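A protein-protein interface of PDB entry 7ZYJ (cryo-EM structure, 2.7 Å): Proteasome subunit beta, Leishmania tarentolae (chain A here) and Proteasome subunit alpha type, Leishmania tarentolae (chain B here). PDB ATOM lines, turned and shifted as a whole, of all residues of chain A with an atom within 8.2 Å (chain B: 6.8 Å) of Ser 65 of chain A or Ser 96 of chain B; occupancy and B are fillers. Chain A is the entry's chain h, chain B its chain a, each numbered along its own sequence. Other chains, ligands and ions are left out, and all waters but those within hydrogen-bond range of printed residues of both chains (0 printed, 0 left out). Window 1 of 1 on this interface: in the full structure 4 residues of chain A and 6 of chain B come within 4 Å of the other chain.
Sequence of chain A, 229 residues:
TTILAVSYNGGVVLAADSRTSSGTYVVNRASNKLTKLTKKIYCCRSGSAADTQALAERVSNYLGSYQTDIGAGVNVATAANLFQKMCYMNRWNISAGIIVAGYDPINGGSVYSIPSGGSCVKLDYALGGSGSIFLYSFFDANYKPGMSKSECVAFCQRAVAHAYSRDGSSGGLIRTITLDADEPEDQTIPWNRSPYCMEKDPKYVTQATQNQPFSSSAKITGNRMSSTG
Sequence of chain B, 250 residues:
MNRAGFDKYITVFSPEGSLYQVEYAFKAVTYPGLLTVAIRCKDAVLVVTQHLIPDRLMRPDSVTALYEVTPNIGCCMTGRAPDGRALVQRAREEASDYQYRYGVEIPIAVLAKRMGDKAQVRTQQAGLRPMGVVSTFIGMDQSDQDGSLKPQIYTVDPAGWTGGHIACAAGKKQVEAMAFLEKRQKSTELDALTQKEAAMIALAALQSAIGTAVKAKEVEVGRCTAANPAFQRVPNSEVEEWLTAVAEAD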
ATOM      1  N   THR A  38     -10.602 -14.895 -15.400  1.00  0.00           N
ATOM      2  CA  THR A  38     -10.053 -13.923 -14.469  1.00  0.00           C
ATOM      3  C   THR A  38      -8.535 -13.927 -14.631  1.00  0.00           C
ATOM      4  O   THR A  38      -7.993 -14.549 -15.548  1.00  0.00           O
ATOM      5  CB  THR A  38     -10.474 -14.229 -13.029  1.00  0.00           C
ATOM      6  OG1 THR A  38      -9.805 -15.409 -12.570  1.00  0.00           O
ATOM      7  CG2 THR A  38     -11.979 -14.432 -12.938  1.00  0.00           C
ATOM      8  N   ARG A  58     -19.338 -14.402 -21.794  1.00  0.00           N
ATOM      9  CA  ARG A  58     -20.397 -14.205 -20.811  1.00  0.00           C
ATOM     10  C   ARG A  58     -19.932 -14.573 -19.408  1.00  0.00           C
ATOM     11  O   ARG A  58     -20.215 -13.852 -18.443  1.00  0.00           O
ATOM     12  CB  ARG A  58     -21.633 -15.013 -21.200  1.00  0.00           C
ATOM     13  CG  ARG A  58     -22.828 -14.798 -20.285  1.00  0.00           C
ATOM     14  CD  ARG A  58     -23.520 -13.478 -20.572  1.00  0.00           C
ATOM     15  NE  ARG A  58     -23.070 -12.425 -19.669  1.00  0.00           N
ATOM     16  CZ  ARG A  58     -23.569 -11.197 -19.641  1.00  0.00           C
ATOM     17  NH1 ARG A  58     -24.540 -10.828 -20.458  1.00  0.00           N
ATOM     18  NH2 ARG A  58     -23.081 -10.319 -18.770  1.00  0.00           N
ATOM     19  N   VAL A  59     -19.208 -15.686 -19.272  1.00  0.00           N
ATOM     20  CA  VAL A  59     -18.742 -16.097 -17.953  1.00  0.00           C
ATOM     21  C   VAL A  59     -17.723 -15.103 -17.409  1.00  0.00           C
ATOM     22  O   VAL A  59     -17.729 -14.780 -16.216  1.00  0.00           O
ATOM     23  CB  VAL A  59     -18.172 -17.526 -18.003  1.00  0.00           C
ATOM     24  CG1 VAL A  59     -17.363 -17.816 -16.751  1.00  0.00           C
ATOM     25  CG2 VAL A  59     -19.294 -18.536 -18.158  1.00  0.00           C
ATOM     26  N   SER A  60     -16.829 -14.607 -18.267  1.00  0.00           N
ATOM     27  CA  SER A  60     -15.847 -13.621 -17.830  1.00  0.00           C
ATOM     28  C   SER A  60     -16.521 -12.327 -17.395  1.00  0.00           C
ATOM     29  O   SER A  60     -16.117 -11.716 -16.398  1.00  0.00           O
ATOM     30  CB  SER A  60     -14.840 -13.355 -18.949  1.00  0.00           C
ATOM     31  OG  SER A  60     -13.850 -12.432 -18.537  1.00  0.00           O
ATOM     32  N   ASN A  61     -17.548 -11.892 -18.129  1.00  0.00           N
ATOM     33  CA  ASN A  61     -18.307 -10.718 -17.714  1.00  0.00           C
ATOM     34  C   ASN A  61     -18.980 -10.945 -16.366  1.00  0.00           C
ATOM     35  O   ASN A  61     -18.971 -10.058 -15.505  1.00  0.00           O
ATOM     36  CB  ASN A  61     -19.343 -10.361 -18.777  1.00  0.00           C
ATOM     37  CG  ASN A  61     -19.974  -9.005 -18.542  1.00  0.00           C
ATOM     38  OD1 ASN A  61     -21.025  -8.900 -17.912  1.00  0.00           O
ATOM     39  ND2 ASN A  61     -19.334  -7.959 -19.046  1.00  0.00           N
ATOM     40  N   TYR A  62     -19.567 -12.127 -16.165  1.00  0.00           N
ATOM     41  CA  TYR A  62     -20.212 -12.426 -14.890  1.00  0.00           C
ATOM     42  C   TYR A  62     -19.205 -12.431 -13.746  1.00  0.00           C
ATOM     43  O   TYR A  62     -19.495 -11.934 -12.652  1.00  0.00           O
ATOM     44  CB  TYR A  62     -20.934 -13.770 -14.973  1.00  0.00           C
ATOM     45  CG  TYR A  62     -22.283 -13.702 -15.646  1.00  0.00           C
ATOM     46  CD1 TYR A  62     -22.914 -12.485 -15.860  1.00  0.00           C
ATOM     47  CD2 TYR A  62     -22.923 -14.856 -16.078  1.00  0.00           C
ATOM     48  CE1 TYR A  62     -24.146 -12.418 -16.478  1.00  0.00           C
ATOM     49  CE2 TYR A  62     -24.156 -14.799 -16.698  1.00  0.00           C
ATOM     50  CZ  TYR A  62     -24.762 -13.578 -16.894  1.00  0.00           C
ATOM     51  OH  TYR A  62     -25.990 -13.515 -17.511  1.00  0.00           O
ATOM     52  N   LEU A  63     -18.019 -12.996 -13.980  1.00  0.00           N
ATOM     53  CA  LEU A  63     -17.020 -13.096 -12.922  1.00  0.00           C
ATOM     54  C   LEU A  63     -16.398 -11.746 -12.598  1.00  0.00           C
ATOM     55  O   LEU A  63     -16.096 -11.472 -11.430  1.00  0.00           O
ATOM     56  CB  LEU A  63     -15.933 -14.092 -13.323  1.00  0.00           C
ATOM     57  CG  LEU A  63     -16.334 -15.567 -13.358  1.00  0.00           C
ATOM     58  CD1 LEU A  63     -15.253 -16.391 -14.035  1.00  0.00           C
ATOM     59  CD2 LEU A  63     -16.615 -16.087 -11.962  1.00  0.00           C
ATOM     60  N   GLY A  64     -16.190 -10.896 -13.606  1.00  0.00           N
ATOM     61  CA  GLY A  64     -15.617  -9.587 -13.351  1.00  0.00           C
ATOM     62  C   GLY A  64     -16.486  -8.720 -12.467  1.00  0.00           C
ATOM     63  O   GLY A  64     -15.977  -8.011 -11.593  1.00  0.00           O
ATOM     64  N   SER A  65     -17.801  -8.760 -12.676  1.00  0.00           N
ATOM     65  CA  SER A  65     -18.723  -8.035 -11.810  1.00  0.00           C
ATOM     66  C   SER A  65     -18.749  -8.631 -10.408  1.00  0.00           C
ATOM     67  O   SER A  65     -18.882  -7.900  -9.422  1.00  0.00           O
ATOM     68  CB  SER A  65     -20.123  -8.044 -12.419  1.00  0.00           C
ATOM     69  OG  SER A  65     -20.173  -7.237 -13.580  1.00  0.00           O
ATOM     70  N   TYR A  66     -18.631  -9.956 -10.308  1.00  0.00           N
ATOM     71  CA  TYR A  66     -18.704 -10.622  -9.013  1.00  0.00           C
ATOM     72  C   TYR A  66     -17.530 -10.229  -8.122  1.00  0.00           C
ATOM     73  O   TYR A  66     -17.691 -10.070  -6.905  1.00  0.00           O
ATOM     74  CB  TYR A  66     -18.762 -12.135  -9.224  1.00  0.00           C
ATOM     75  CG  TYR A  66     -18.785 -12.959  -7.960  1.00  0.00           C
ATOM     76  CD1 TYR A  66     -19.950 -13.087  -7.217  1.00  0.00           C
ATOM     77  CD2 TYR A  66     -17.654 -13.631  -7.523  1.00  0.00           C
ATOM     78  CE1 TYR A  66     -19.983 -13.847  -6.067  1.00  0.00           C
ATOM     79  CE2 TYR A  66     -17.677 -14.395  -6.374  1.00  0.00           C
ATOM     80  CZ  TYR A  66     -18.844 -14.499  -5.650  1.00  0.00           C
ATOM     81  OH  TYR A  66     -18.870 -15.258  -4.504  1.00  0.00           O
ATOM     82  N   GLN A  67     -16.338 -10.066  -8.710  1.00  0.00           N
ATOM     83  CA  GLN A  67     -15.187  -9.608  -7.936  1.00  0.00           C
ATOM     84  C   GLN A  67     -15.432  -8.228  -7.347  1.00  0.00           C
ATOM     85  O   GLN A  67     -15.110  -7.977  -6.180  1.00  0.00           O
ATOM     86  CB  GLN A  67     -13.933  -9.566  -8.807  1.00  0.00           C
ATOM     87  CG  GLN A  67     -13.429 -10.902  -9.285  1.00  0.00           C
ATOM     88  CD  GLN A  67     -12.197 -10.772 -10.153  1.00  0.00           C
ATOM     89  OE1 GLN A  67     -11.752  -9.665 -10.453  1.00  0.00           O
ATOM     90  NE2 GLN A  67     -11.640 -11.904 -10.566  1.00  0.00           N
ATOM     91  N   THR A  68     -15.986  -7.316  -8.146  1.00  0.00           N
ATOM     92  CA  THR A  68     -16.289  -5.981  -7.647  1.00  0.00           C
ATOM     93  C   THR A  68     -17.360  -6.021  -6.568  1.00  0.00           C
ATOM     94  O   THR A  68     -17.271  -5.289  -5.575  1.00  0.00           O
ATOM     95  CB  THR A  68     -16.727  -5.082  -8.801  1.00  0.00           C
ATOM     96  OG1 THR A  68     -15.682  -5.014  -9.777  1.00  0.00           O
ATOM     97  CG2 THR A  68     -17.023  -3.686  -8.300  1.00  0.00           C
ATOM     98  N   ASP A  69     -18.372  -6.872  -6.739  1.00  0.00           N
ATOM     99  CA  ASP A  69     -19.441  -6.969  -5.752  1.00  0.00           C
ATOM    100  C   ASP A  69     -18.920  -7.479  -4.414  1.00  0.00           C
ATOM    101  O   ASP A  69     -19.202  -6.893  -3.364  1.00  0.00           O
ATOM    102  CB  ASP A  69     -20.553  -7.875  -6.276  1.00  0.00           C
ATOM    103  CG  ASP A  69     -21.765  -7.888  -5.371  1.00  0.00           C
ATOM    104  OD1 ASP A  69     -22.080  -6.832  -4.784  1.00  0.00           O
ATOM    105  OD2 ASP A  69     -22.408  -8.952  -5.250  1.00  0.00           O
ATOM    106  N   ILE A  70     -18.157  -8.575  -4.428  1.00  0.00           N
ATOM    107  CA  ILE A  70     -17.694  -9.143  -3.165  1.00  0.00           C
ATOM    108  C   ILE A  70     -16.401  -8.503  -2.679  1.00  0.00           C
ATOM    109  O   ILE A  70     -16.076  -8.614  -1.492  1.00  0.00           O
ATOM    110  CB  ILE A  70     -17.503 -10.666  -3.269  1.00  0.00           C
ATOM    111  CG1 ILE A  70     -16.290 -11.000  -4.139  1.00  0.00           C
ATOM    112  CG2 ILE A  70     -18.760 -11.324  -3.818  1.00  0.00           C
ATOM    113  CD1 ILE A  70     -15.884 -12.451  -4.084  1.00  0.00           C
ATOM    114  N   GLY A  71     -15.657  -7.834  -3.555  1.00  0.00           N
ATOM    115  CA  GLY A  71     -14.413  -7.217  -3.142  1.00  0.00           C
ATOM    116  C   GLY A  71     -13.302  -8.186  -2.821  1.00  0.00           C
ATOM    117  O   GLY A  71     -12.368  -7.825  -2.101  1.00  0.00           O
ATOM    118  N   ALA A  72     -13.376  -9.414  -3.331  1.00  0.00           N
ATOM    119  CA  ALA A  72     -12.353 -10.424  -3.101  1.00  0.00           C
ATOM    120  C   ALA A  72     -12.136 -11.200  -4.393  1.00  0.00           C
ATOM    121  O   ALA A  72     -12.727 -10.895  -5.433  1.00  0.00           O
ATOM    122  CB  ALA A  72     -12.741 -11.357  -1.949  1.00  0.00           C
ATOM    123  N   VAL A  74     -12.020 -14.753  -6.832  1.00  0.00           N
ATOM    124  CA  VAL A  74     -12.983 -15.780  -7.213  1.00  0.00           C
ATOM    125  C   VAL A  74     -12.297 -17.135  -7.207  1.00  0.00           C
ATOM    126  O   VAL A  74     -11.187 -17.287  -7.732  1.00  0.00           O
ATOM    127  CB  VAL A  74     -13.600 -15.478  -8.591  1.00  0.00           C
ATOM    128  CG1 VAL A  74     -14.580 -16.567  -8.981  1.00  0.00           C
ATOM    129  CG2 VAL A  74     -14.288 -14.137  -8.570  1.00  0.00           C
ATOM    130  N   VAL B  69     -16.168   1.081  -8.798  1.00  0.00           N
ATOM    131  CA  VAL B  69     -17.117   0.839  -9.880  1.00  0.00           C
ATOM    132  C   VAL B  69     -16.541  -0.166 -10.864  1.00  0.00           C
ATOM    133  O   VAL B  69     -17.132  -1.219 -11.129  1.00  0.00           O
ATOM    134  CB  VAL B  69     -17.491   2.158 -10.578  1.00  0.00           C
ATOM    135  CG1 VAL B  69     -18.430   1.888 -11.742  1.00  0.00           C
ATOM    136  CG2 VAL B  69     -18.128   3.113  -9.591  1.00  0.00           C
ATOM    137  N   THR B  70     -15.379   0.147 -11.416  1.00  0.00           N
ATOM    138  CA  THR B  70     -14.586  -0.768 -12.219  1.00  0.00           C
ATOM    139  C   THR B  70     -13.170  -0.724 -11.674  1.00  0.00           C
ATOM    140  O   THR B  70     -12.804   0.218 -10.963  1.00  0.00           O
ATOM    141  CB  THR B  70     -14.586  -0.388 -13.708  1.00  0.00           C
ATOM    142  OG1 THR B  70     -13.879   0.842 -13.891  1.00  0.00           O
ATOM    143  CG2 THR B  70     -16.003  -0.229 -14.224  1.00  0.00           C
ATOM    144  N   ARG B  90     -26.147   0.628  -9.319  1.00  0.00           N
ATOM    145  CA  ARG B  90     -26.570   0.886 -10.692  1.00  0.00           C
ATOM    146  C   ARG B  90     -25.366   1.072 -11.599  1.00  0.00           C
ATOM    147  O   ARG B  90     -25.275   0.444 -12.664  1.00  0.00           O
ATOM    148  CB  ARG B  90     -27.481   2.114 -10.750  1.00  0.00           C
ATOM    149  CG  ARG B  90     -28.534   2.193  -9.655  1.00  0.00           C
ATOM    150  CD  ARG B  90     -29.809   1.450 -10.035  1.00  0.00           C
ATOM    151  NE  ARG B  90     -29.610   0.010 -10.132  1.00  0.00           N
ATOM    152  CZ  ARG B  90     -29.564  -0.813  -9.093  1.00  0.00           C
ATOM    153  NH1 ARG B  90     -29.715  -0.372  -7.854  1.00  0.00           N
ATOM    154  NH2 ARG B  90     -29.361  -2.110  -9.301  1.00  0.00           N
ATOM    155  N   ALA B  91     -24.396   1.878 -11.155  1.00  0.00           N
ATOM    156  CA  ALA B  91     -23.240   2.173 -11.994  1.00  0.00           C
ATOM    157  C   ALA B  91     -22.583   0.885 -12.459  1.00  0.00           C
ATOM    158  O   ALA B  91     -22.198   0.752 -13.628  1.00  0.00           O
ATOM    159  CB  ALA B  91     -22.244   3.048 -11.230  1.00  0.00           C
ATOM    160  N   ARG B  92     -22.522  -0.105 -11.568  1.00  0.00           N
ATOM    161  CA  ARG B  92     -21.847  -1.351 -11.897  1.00  0.00           C
ATOM    162  C   ARG B  92     -22.503  -2.034 -13.091  1.00  0.00           C
ATOM    163  O   ARG B  92     -21.813  -2.408 -14.048  1.00  0.00           O
ATOM    164  CB  ARG B  92     -21.808  -2.255 -10.667  1.00  0.00           C
ATOM    165  CG  ARG B  92     -20.818  -1.738  -9.634  1.00  0.00           C
ATOM    166  CD  ARG B  92     -20.902  -2.455  -8.305  1.00  0.00           C
ATOM    167  NE  ARG B  92     -19.790  -2.070  -7.444  1.00  0.00           N
ATOM    168  CZ  ARG B  92     -19.695  -2.366  -6.156  1.00  0.00           C
ATOM    169  NH1 ARG B  92     -20.638  -3.055  -5.534  1.00  0.00           N
ATOM    170  NH2 ARG B  92     -18.629  -1.960  -5.475  1.00  0.00           N
ATOM    171  N   GLU B  93     -23.839  -2.151 -13.098  1.00  0.00           N
ATOM    172  CA  GLU B  93     -24.463  -2.713 -14.293  1.00  0.00           C
ATOM    173  C   GLU B  93     -24.180  -1.835 -15.499  1.00  0.00           C
ATOM    174  O   GLU B  93     -23.827  -2.339 -16.572  1.00  0.00           O
ATOM    175  CB  GLU B  93     -25.975  -2.916 -14.142  1.00  0.00           C
ATOM    176  CG  GLU B  93     -26.413  -3.974 -13.143  1.00  0.00           C
ATOM    177  CD  GLU B  93     -26.451  -3.454 -11.739  1.00  0.00           C
ATOM    178  OE1 GLU B  93     -26.200  -2.251 -11.578  1.00  0.00           O
ATOM    179  OE2 GLU B  93     -26.725  -4.237 -10.806  1.00  0.00           O
ATOM    180  N   GLU B  94     -24.275  -0.514 -15.326  1.00  0.00           N
ATOM    181  CA  GLU B  94     -24.026   0.374 -16.452  1.00  0.00           C
ATOM    182  C   GLU B  94     -22.594   0.235 -16.939  1.00  0.00           C
ATOM    183  O   GLU B  94     -22.295   0.553 -18.095  1.00  0.00           O
ATOM    184  CB  GLU B  94     -24.341   1.819 -16.070  1.00  0.00           C
ATOM    185  CG  GLU B  94     -24.511   2.756 -17.260  1.00  0.00           C
ATOM    186  CD  GLU B  94     -25.845   2.574 -17.979  1.00  0.00           C
ATOM    187  OE1 GLU B  94     -26.468   1.499 -17.854  1.00  0.00           O
ATOM    188  OE2 GLU B  94     -26.280   3.515 -18.670  1.00  0.00           O
ATOM    189  N   ALA B  95     -21.697  -0.246 -16.077  1.00  0.00           N
ATOM    190  CA  ALA B  95     -20.382  -0.651 -16.549  1.00  0.00           C
ATOM    191  C   ALA B  95     -20.442  -2.039 -17.173  1.00  0.00           C
ATOM    192  O   ALA B  95     -20.072  -2.223 -18.339  1.00  0.00           O
ATOM    193  CB  ALA B  95     -19.378  -0.614 -15.400  1.00  0.00           C
ATOM    194  N   SER B  96     -20.963  -3.014 -16.424  1.00  0.00           N
ATOM    195  CA  SER B  96     -20.916  -4.407 -16.857  1.00  0.00           C
ATOM    196  C   SER B  96     -21.609  -4.586 -18.199  1.00  0.00           C
ATOM    197  O   SER B  96     -21.023  -5.119 -19.151  1.00  0.00           O
ATOM    198  CB  SER B  96     -21.554  -5.304 -15.796  1.00  0.00           C
ATOM    199  OG  SER B  96     -21.025  -5.030 -14.512  1.00  0.00           O
ATOM    200  N   ASP B  97     -22.853  -4.111 -18.304  1.00  0.00           N
ATOM    201  CA  ASP B  97     -23.568  -4.183 -19.572  1.00  0.00           C
ATOM    202  C   ASP B  97     -22.754  -3.531 -20.680  1.00  0.00           C
ATOM    203  O   ASP B  97     -22.587  -4.104 -21.763  1.00  0.00           O
ATOM    204  CB  ASP B  97     -24.939  -3.518 -19.443  1.00  0.00           C
ATOM    205  CG  ASP B  97     -25.752  -4.076 -18.293  1.00  0.00           C
ATOM    206  OD1 ASP B  97     -25.358  -5.123 -17.738  1.00  0.00           O
ATOM    207  OD2 ASP B  97     -26.786  -3.470 -17.945  1.00  0.00           O
ATOM    208  N   TYR B  98     -22.197  -2.349 -20.402  1.00  0.00           N
ATOM    209  CA  TYR B  98     -21.347  -1.689 -21.385  1.00  0.00           C
ATOM    210  C   TYR B  98     -20.200  -2.601 -21.790  1.00  0.00           C
ATOM    211  O   TYR B  98     -19.951  -2.817 -22.983  1.00  0.00           O
ATOM    212  CB  TYR B  98     -20.822  -0.371 -20.815  1.00  0.00           C
ATOM    213  CG  TYR B  98     -20.115   0.514 -21.819  1.00  0.00           C
ATOM    214  CD1 TYR B  98     -18.796   0.274 -22.180  1.00  0.00           C
ATOM    215  CD2 TYR B  98     -20.762   1.599 -22.392  1.00  0.00           C
ATOM    216  CE1 TYR B  98     -18.148   1.078 -23.088  1.00  0.00           C
ATOM    217  CE2 TYR B  98     -20.119   2.411 -23.303  1.00  0.00           C
ATOM    218  CZ  TYR B  98     -18.812   2.145 -23.646  1.00  0.00           C
ATOM    219  OH  TYR B  98     -18.164   2.949 -24.553  1.00  0.00           O
ATOM    220  N   GLN B  99     -19.525  -3.191 -20.800  1.00  0.00           N
ATOM    221  CA  GLN B  99     -18.426  -4.102 -21.093  1.00  0.00           C
ATOM    222  C   GLN B  99     -18.898  -5.263 -21.954  1.00  0.00           C
ATOM    223  O   GLN B  99     -18.172  -5.727 -22.840  1.00  0.00           O
ATOM    224  CB  GLN B  99     -17.805  -4.605 -19.789  1.00  0.00           C
ATOM    225  CG  GLN B  99     -16.941  -5.843 -19.939  1.00  0.00           C
ATOM    226  CD  GLN B  99     -15.675  -5.576 -20.723  1.00  0.00           C
ATOM    227  OE1 GLN B  99     -15.041  -4.534 -20.563  1.00  0.00           O
ATOM    228  NE2 GLN B  99     -15.299  -6.519 -21.578  1.00  0.00           N
ATOM    229  N   TYR B 100     -20.124  -5.734 -21.726  1.00  0.00           N
ATOM    230  CA  TYR B 100     -20.623  -6.859 -22.500  1.00  0.00           C
ATOM    231  C   TYR B 100     -21.124  -6.445 -23.876  1.00  0.00           C
ATOM    232  O   TYR B 100     -21.262  -7.304 -24.751  1.00  0.00           O
ATOM    233  CB  TYR B 100     -21.730  -7.580 -21.725  1.00  0.00           C
ATOM    234  CG  TYR B 100     -22.235  -8.835 -22.399  1.00  0.00           C
ATOM    235  CD1 TYR B 100     -21.577 -10.045 -22.233  1.00  0.00           C
ATOM    236  CD2 TYR B 100     -23.381  -8.815 -23.185  1.00  0.00           C
ATOM    237  CE1 TYR B 100     -22.031 -11.195 -22.843  1.00  0.00           C
ATOM    238  CE2 TYR B 100     -23.843  -9.961 -23.798  1.00  0.00           C
ATOM    239  CZ  TYR B 100     -23.166 -11.148 -23.623  1.00  0.00           C
ATOM    240  OH  TYR B 100     -23.627 -12.292 -24.231  1.00  0.00           O
ATOM    241  N   ARG B 101     -21.375  -5.155 -24.105  1.00  0.00           N
ATOM    242  CA  ARG B 101     -21.919  -4.755 -25.396  1.00  0.00           C
ATOM    243  C   ARG B 101     -20.860  -4.213 -26.343  1.00  0.00           C
ATOM    244  O   ARG B 101     -21.030  -4.304 -27.565  1.00  0.00           O
ATOM    245  CB  ARG B 101     -23.026  -3.715 -25.211  1.00  0.00           C
ATOM    246  CG  ARG B 101     -24.248  -4.251 -24.481  1.00  0.00           C
ATOM    247  CD  ARG B 101     -25.310  -3.179 -24.307  1.00  0.00           C
ATOM    248  NE  ARG B 101     -25.876  -2.769 -25.585  1.00  0.00           N
ATOM    249  CZ  ARG B 101     -25.664  -1.591 -26.157  1.00  0.00           C
ATOM    250  NH1 ARG B 101     -24.901  -0.673 -25.587  1.00  0.00           N
ATOM    251  NH2 ARG B 101     -26.232  -1.329 -27.330  1.00  0.00           N
ATOM    252  N   ILE B 106     -15.770   0.749 -19.815  1.00  0.00           N
ATOM    253  CA  ILE B 106     -16.539   1.983 -20.015  1.00  0.00           C
ATOM    254  C   ILE B 106     -15.673   3.188 -19.669  1.00  0.00           C
ATOM    255  O   ILE B 106     -14.943   3.157 -18.661  1.00  0.00           O
ATOM    256  CB  ILE B 106     -17.823   1.954 -19.176  1.00  0.00           C
ATOM    257  CG1 ILE B 106     -18.712   3.154 -19.511  1.00  0.00           C
ATOM    258  CG2 ILE B 106     -17.518   1.889 -17.684  1.00  0.00           C
ATOM    259  CD1 ILE B 106     -20.121   3.033 -18.981  1.00  0.00           C
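The side-chain amide nitrogen of Asn 61 of chain A lies within hydrogen-bond range of the backbone carbonyl oxygen of Ser 96 of chain B. The side-chain hydroxyl of Ser 96 of chain B is in hydrogen-bond range of the side-chain hydroxyl of Ser 65 of chain A, 2.5 Å away.
The guanidinium group of Arg 58 of chain A sits at hydrogen-bond distance from the side-chain amide oxygen of Asn 61 of chain A, 2.6 Å away. OG of Ser 96 of chain B lies within hydrogen-bond range of O of Arg 92 of chain B.
NH1 of Arg 58 of chain A touches CZ of Tyr 100 of chain B, 3.5 Å away. Gln 99 of chain B touches Asn 61 of chain A. N of Tyr 100 of chain B touches ND2 of Asn 61 of chain A (3.6 Å). Thr 68 of chain A touches Val 69 of chain B. Thr 68 of chain A touches Arg 92 of chain B (CG2 to NE, 3.3 Å).
Ser 65 of chain A touches just one residue of chain B: Ser 96 (2.5 Å). Asp 69 of chain A touches none of the printed residues of chain B. Printed residues of chain A within 4 Å of Arg 92 of chain B: Thr 68 (3.3 Å). No residue of chain A comes within 4 Å of Ala 95 of chain B. Ser 96 of chain B touches just these residues of chain A: Asn 61 (3.3 Å) and Ser 65 (2.5 Å). Printed residues of chain A within 4 Å of Tyr 100 of chain B: Arg 58 (3.5 Å) and Asn 61 (3.6 Å). The nearest printed residue of chain B that does not touch Thr 68 of chain A is Thr 70 of chain B (5.0 Å).
Hydrophobic or aromatic side chains of chain B within 4 Å of the printed part of chain A: Tyr 100. Among the printed residues, 7 pairs touch across the chains. Among the printed residues, no Asp or Glu carboxylate lies within 4 Å of a Lys or Arg side-chain nitrogen of the other chain.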
